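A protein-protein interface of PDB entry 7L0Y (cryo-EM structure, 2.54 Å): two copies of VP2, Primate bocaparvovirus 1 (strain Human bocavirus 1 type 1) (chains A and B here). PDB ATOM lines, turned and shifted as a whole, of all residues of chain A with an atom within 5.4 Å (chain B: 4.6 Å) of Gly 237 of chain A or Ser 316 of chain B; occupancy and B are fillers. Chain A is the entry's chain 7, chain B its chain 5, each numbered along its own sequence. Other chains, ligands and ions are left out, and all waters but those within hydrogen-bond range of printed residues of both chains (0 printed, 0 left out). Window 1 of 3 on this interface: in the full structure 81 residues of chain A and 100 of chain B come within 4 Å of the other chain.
The backbone NH (N) of Phe 318 of chain B is in hydrogen-bond range of the backbone carbonyl oxygen (O) of Phe 296 of chain B, 2.7 Å away. N of Gly 317 of chain B is in hydrogen-bond range of SD of Met 297 of chain B, 3.7 Å away. The backbone NH (N) of Val 298 of chain B sits at hydrogen-bond distance from the backbone carbonyl oxygen (O) of Ser 316 of chain B, at 2.6 Å. The side-chain carboxylate (OD2) of Asp 292 of chain B is in hydrogen-bond range of the backbone NH (N) of Gly 317 of chain B.
No position is printed for both chains.
Of the 9 printed residues of chain B, 3 touch a printed residue of chain A. Among the printed residues, no Asp or Glu carboxylate lies within 4 Å of a Lys or Arg side-chain nitrogen of the other chain.
Gly 237 of chain A touches Ser 316 of chain B (O to OG, 3.5 Å). Gly 317 of chain B touches Pro 271 of chain A. Phe 318 of chain B touches Thr 272 of chain A (CD1 to O, 3.7 Å).
N of Thr 272 of chain A lies within hydrogen-bond range of O of Gly 317 of chain B (2.9 Å). The side-chain hydroxyl (OG) of Ser 316 of chain B lies within hydrogen-bond range of the backbone carbonyl oxygen (O) of Lys 270 of chain A (3.0 Å).
Of chain B, only Ser 316 (3.5 Å) comes within 4 Å of Gly 237 of chain A. Ser 316 of chain B touches just these residues of chain A: Gly 237 and Lys 270. Printed residues of chain B within 4 Å of Lys 270 of chain A: Ser 316 (3.0 Å). Printed residues of chain B within 4 Å of Pro 271 of chain A: Gly 317. The nearest residue of chain A that does not touch Ser 316 of chain B is Thr 272 of chain A (4.1 Å). The nearest printed residue of chain B that does not touch Pro 271 of chain A is Ser 316 of chain B (4.6 Å).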
ATOM      1  N   PRO A 235      -2.195 -26.373 -14.091  1.00  0.00           N
ATOM      2  CA  PRO A 235      -1.089 -26.993 -13.380  1.00  0.00           C
ATOM      3  C   PRO A 235      -1.453 -28.406 -12.972  1.00  0.00           C
ATOM      4  O   PRO A 235      -2.641 -28.759 -12.895  1.00  0.00           O
ATOM      5  CB  PRO A 235      -0.913 -26.087 -12.151  1.00  0.00           C
ATOM      6  CG  PRO A 235      -1.502 -24.812 -12.552  1.00  0.00           C
ATOM      7  CD  PRO A 235      -2.652 -25.148 -13.424  1.00  0.00           C
ATOM      8  N   PRO A 236      -0.464 -29.254 -12.695  1.00  0.00           N
ATOM      9  CA  PRO A 236      -0.780 -30.583 -12.163  1.00  0.00           C
ATOM     10  C   PRO A 236      -1.455 -30.542 -10.808  1.00  0.00           C
ATOM     11  O   PRO A 236      -2.017 -31.557 -10.384  1.00  0.00           O
ATOM     12  CB  PRO A 236       0.590 -31.267 -12.096  1.00  0.00           C
ATOM     13  CG  PRO A 236       1.549 -30.156 -12.013  1.00  0.00           C
ATOM     14  CD  PRO A 236       0.982 -29.057 -12.844  1.00  0.00           C
ATOM     15  N   GLY A 237      -1.422 -29.404 -10.116  1.00  0.00           N
ATOM     16  CA  GLY A 237      -2.051 -29.322  -8.812  1.00  0.00           C
ATOM     17  C   GLY A 237      -3.551 -29.132  -8.869  1.00  0.00           C
ATOM     18  O   GLY A 237      -4.238 -29.300  -7.863  1.00  0.00           O
ATOM     19  N   LEU A 238      -4.081 -28.770 -10.030  1.00  0.00           N
ATOM     20  CA  LEU A 238      -5.509 -28.550 -10.209  1.00  0.00           C
ATOM     21  C   LEU A 238      -6.253 -29.760 -10.748  1.00  0.00           C
ATOM     22  O   LEU A 238      -7.427 -29.634 -11.101  1.00  0.00           O
ATOM     23  CB  LEU A 238      -5.757 -27.344 -11.109  1.00  0.00           C
ATOM     24  CG  LEU A 238      -5.449 -26.020 -10.428  1.00  0.00           C
ATOM     25  CD1 LEU A 238      -5.691 -24.873 -11.375  1.00  0.00           C
ATOM     26  CD2 LEU A 238      -6.295 -25.888  -9.185  1.00  0.00           C
ATOM     27  N   MET A 239      -5.607 -30.921 -10.831  1.00  0.00           N
ATOM     28  CA  MET A 239      -6.219 -32.070 -11.488  1.00  0.00           C
ATOM     29  C   MET A 239      -7.412 -32.630 -10.724  1.00  0.00           C
ATOM     30  O   MET A 239      -7.978 -33.638 -11.145  1.00  0.00           O
ATOM     31  CB  MET A 239      -5.201 -33.184 -11.710  1.00  0.00           C
ATOM     32  CG  MET A 239      -4.089 -32.852 -12.678  1.00  0.00           C
ATOM     33  SD  MET A 239      -3.137 -34.318 -13.121  1.00  0.00           S
ATOM     34  CE  MET A 239      -2.312 -34.703 -11.576  1.00  0.00           C
ATOM     35  N   PHE A 240      -7.774 -32.053  -9.590  1.00  0.00           N
ATOM     36  CA  PHE A 240      -8.862 -32.615  -8.812  1.00  0.00           C
ATOM     37  C   PHE A 240     -10.218 -32.047  -9.232  1.00  0.00           C
ATOM     38  O   PHE A 240     -10.332 -31.175 -10.093  1.00  0.00           O
ATOM     39  CB  PHE A 240      -8.625 -32.355  -7.331  1.00  0.00           C
ATOM     40  CG  PHE A 240      -8.515 -30.911  -6.992  1.00  0.00           C
ATOM     41  CD1 PHE A 240      -9.628 -30.190  -6.614  1.00  0.00           C
ATOM     42  CD2 PHE A 240      -7.298 -30.268  -7.062  1.00  0.00           C
ATOM     43  CE1 PHE A 240      -9.525 -28.871  -6.303  1.00  0.00           C
ATOM     44  CE2 PHE A 240      -7.194 -28.942  -6.753  1.00  0.00           C
ATOM     45  CZ  PHE A 240      -8.305 -28.245  -6.374  1.00  0.00           C
ATOM     46  N   LYS A 270      -7.322 -29.140  -2.918  1.00  0.00           N
ATOM     47  CA  LYS A 270      -6.851 -30.455  -2.512  1.00  0.00           C
ATOM     48  C   LYS A 270      -5.328 -30.531  -2.563  1.00  0.00           C
ATOM     49  O   LYS A 270      -4.707 -29.959  -3.460  1.00  0.00           O
ATOM     50  CB  LYS A 270      -7.477 -31.535  -3.376  1.00  0.00           C
ATOM     51  CG  LYS A 270      -8.946 -31.673  -3.084  1.00  0.00           C
ATOM     52  CD  LYS A 270      -9.610 -32.688  -3.953  1.00  0.00           C
ATOM     53  CE  LYS A 270     -11.068 -32.795  -3.602  1.00  0.00           C
ATOM     54  NZ  LYS A 270     -11.781 -33.726  -4.495  1.00  0.00           N
ATOM     55  N   PRO A 271      -4.705 -31.216  -1.605  1.00  0.00           N
ATOM     56  CA  PRO A 271      -3.245 -31.353  -1.627  1.00  0.00           C
ATOM     57  C   PRO A 271      -2.776 -32.052  -2.888  1.00  0.00           C
ATOM     58  O   PRO A 271      -3.416 -32.980  -3.381  1.00  0.00           O
ATOM     59  CB  PRO A 271      -2.953 -32.204  -0.389  1.00  0.00           C
ATOM     60  CG  PRO A 271      -4.134 -32.037   0.477  1.00  0.00           C
ATOM     61  CD  PRO A 271      -5.302 -31.894  -0.445  1.00  0.00           C
ATOM     62  N   THR A 272      -1.639 -31.612  -3.404  1.00  0.00           N
ATOM     63  CA  THR A 272      -1.047 -32.230  -4.576  1.00  0.00           C
ATOM     64  C   THR A 272       0.216 -32.977  -4.177  1.00  0.00           C
ATOM     65  O   THR A 272       0.891 -32.629  -3.206  1.00  0.00           O
ATOM     66  CB  THR A 272      -0.732 -31.196  -5.669  1.00  0.00           C
ATOM     67  OG1 THR A 272      -0.356 -31.873  -6.873  1.00  0.00           O
ATOM     68  CG2 THR A 272       0.399 -30.268  -5.246  1.00  0.00           C
ATOM     69  N   ASP B 292      -6.491 -22.565   1.818  1.00  0.00           N
ATOM     70  CA  ASP B 292      -5.565 -23.647   1.518  1.00  0.00           C
ATOM     71  C   ASP B 292      -4.323 -23.425   2.367  1.00  0.00           C
ATOM     72  O   ASP B 292      -3.571 -22.473   2.149  1.00  0.00           O
ATOM     73  CB  ASP B 292      -5.244 -23.679   0.027  1.00  0.00           C
ATOM     74  CG  ASP B 292      -4.318 -24.812  -0.347  1.00  0.00           C
ATOM     75  OD1 ASP B 292      -4.626 -25.979  -0.036  1.00  0.00           O
ATOM     76  OD2 ASP B 292      -3.298 -24.544  -1.001  1.00  0.00           O
ATOM     77  N   PHE B 296       3.737 -25.611   1.871  1.00  0.00           N
ATOM     78  CA  PHE B 296       4.307 -25.217   0.596  1.00  0.00           C
ATOM     79  C   PHE B 296       3.190 -25.014  -0.407  1.00  0.00           C
ATOM     80  O   PHE B 296       2.253 -25.812  -0.474  1.00  0.00           O
ATOM     81  CB  PHE B 296       5.303 -26.247   0.081  1.00  0.00           C
ATOM     82  CG  PHE B 296       6.562 -26.289   0.865  1.00  0.00           C
ATOM     83  CD1 PHE B 296       7.566 -25.384   0.610  1.00  0.00           C
ATOM     84  CD2 PHE B 296       6.739 -27.214   1.868  1.00  0.00           C
ATOM     85  CE1 PHE B 296       8.722 -25.407   1.326  1.00  0.00           C
ATOM     86  CE2 PHE B 296       7.898 -27.239   2.593  1.00  0.00           C
ATOM     87  CZ  PHE B 296       8.893 -26.334   2.321  1.00  0.00           C
ATOM     88  N   MET B 297       3.296 -23.949  -1.181  1.00  0.00           N
ATOM     89  CA  MET B 297       2.300 -23.599  -2.174  1.00  0.00           C
ATOM     90  C   MET B 297       2.967 -23.655  -3.539  1.00  0.00           C
ATOM     91  O   MET B 297       3.922 -22.917  -3.794  1.00  0.00           O
ATOM     92  CB  MET B 297       1.734 -22.213  -1.892  1.00  0.00           C
ATOM     93  CG  MET B 297       0.490 -21.911  -2.652  1.00  0.00           C
ATOM     94  SD  MET B 297      -0.831 -22.997  -2.106  1.00  0.00           S
ATOM     95  CE  MET B 297      -1.049 -22.429  -0.423  1.00  0.00           C
ATOM     96  N   VAL B 298       2.472 -24.530  -4.404  1.00  0.00           N
ATOM     97  CA  VAL B 298       3.057 -24.755  -5.719  1.00  0.00           C
ATOM     98  C   VAL B 298       2.235 -23.970  -6.724  1.00  0.00           C
ATOM     99  O   VAL B 298       1.132 -24.385  -7.088  1.00  0.00           O
ATOM    100  CB  VAL B 298       3.074 -26.252  -6.069  1.00  0.00           C
ATOM    101  CG1 VAL B 298       3.562 -26.472  -7.479  1.00  0.00           C
ATOM    102  CG2 VAL B 298       3.925 -27.023  -5.080  1.00  0.00           C
ATOM    103  N   PHE B 314      -3.626 -18.582  -6.747  1.00  0.00           N
ATOM    104  CA  PHE B 314      -2.454 -19.120  -7.418  1.00  0.00           C
ATOM    105  C   PHE B 314      -2.044 -20.425  -6.763  1.00  0.00           C
ATOM    106  O   PHE B 314      -1.875 -20.501  -5.543  1.00  0.00           O
ATOM    107  CB  PHE B 314      -1.288 -18.137  -7.360  1.00  0.00           C
ATOM    108  CG  PHE B 314      -1.551 -16.832  -8.044  1.00  0.00           C
ATOM    109  CD1 PHE B 314      -1.492 -16.736  -9.420  1.00  0.00           C
ATOM    110  CD2 PHE B 314      -1.810 -15.691  -7.310  1.00  0.00           C
ATOM    111  CE1 PHE B 314      -1.723 -15.536 -10.052  1.00  0.00           C
ATOM    112  CE2 PHE B 314      -2.029 -14.484  -7.939  1.00  0.00           C
ATOM    113  CZ  PHE B 314      -1.989 -14.408  -9.312  1.00  0.00           C
ATOM    114  N   GLY B 315      -1.906 -21.452  -7.573  1.00  0.00           N
ATOM    115  CA  GLY B 315      -1.271 -22.654  -7.113  1.00  0.00           C
ATOM    116  C   GLY B 315      -2.066 -23.496  -6.134  1.00  0.00           C
ATOM    117  O   GLY B 315      -3.140 -23.141  -5.655  1.00  0.00           O
ATOM    118  N   SER B 316      -1.483 -24.654  -5.844  1.00  0.00           N
ATOM    119  CA  SER B 316      -2.072 -25.639  -4.957  1.00  0.00           C
ATOM    120  C   SER B 316      -1.062 -25.952  -3.867  1.00  0.00           C
ATOM    121  O   SER B 316       0.135 -25.700  -4.010  1.00  0.00           O
ATOM    122  CB  SER B 316      -2.469 -26.904  -5.722  1.00  0.00           C
ATOM    123  OG  SER B 316      -3.003 -27.890  -4.862  1.00  0.00           O
ATOM    124  N   GLY B 317      -1.555 -26.517  -2.767  1.00  0.00           N
ATOM    125  CA  GLY B 317      -0.706 -26.830  -1.640  1.00  0.00           C
ATOM    126  C   GLY B 317       0.002 -28.157  -1.807  1.00  0.00           C
ATOM    127  O   GLY B 317      -0.567 -29.113  -2.338  1.00  0.00           O
ATOM    128  N   PHE B 318       1.243 -28.217  -1.338  1.00  0.00           N
ATOM    129  CA  PHE B 318       2.051 -29.426  -1.418  1.00  0.00           C
ATOM    130  C   PHE B 318       2.111 -30.023  -0.018  1.00  0.00           C
ATOM    131  O   PHE B 318       2.791 -29.511   0.870  1.00  0.00           O
ATOM    132  CB  PHE B 318       3.434 -29.105  -1.962  1.00  0.00           C
ATOM    133  CG  PHE B 318       4.322 -30.295  -2.086  1.00  0.00           C
ATOM    134  CD1 PHE B 318       4.264 -31.099  -3.206  1.00  0.00           C
ATOM    135  CD2 PHE B 318       5.200 -30.623  -1.077  1.00  0.00           C
ATOM    136  CE1 PHE B 318       5.076 -32.193  -3.320  1.00  0.00           C
ATOM    137  CE2 PHE B 318       6.010 -31.718  -1.186  1.00  0.00           C
ATOM    138  CZ  PHE B 318       5.949 -32.504  -2.309  1.00  0.00           C
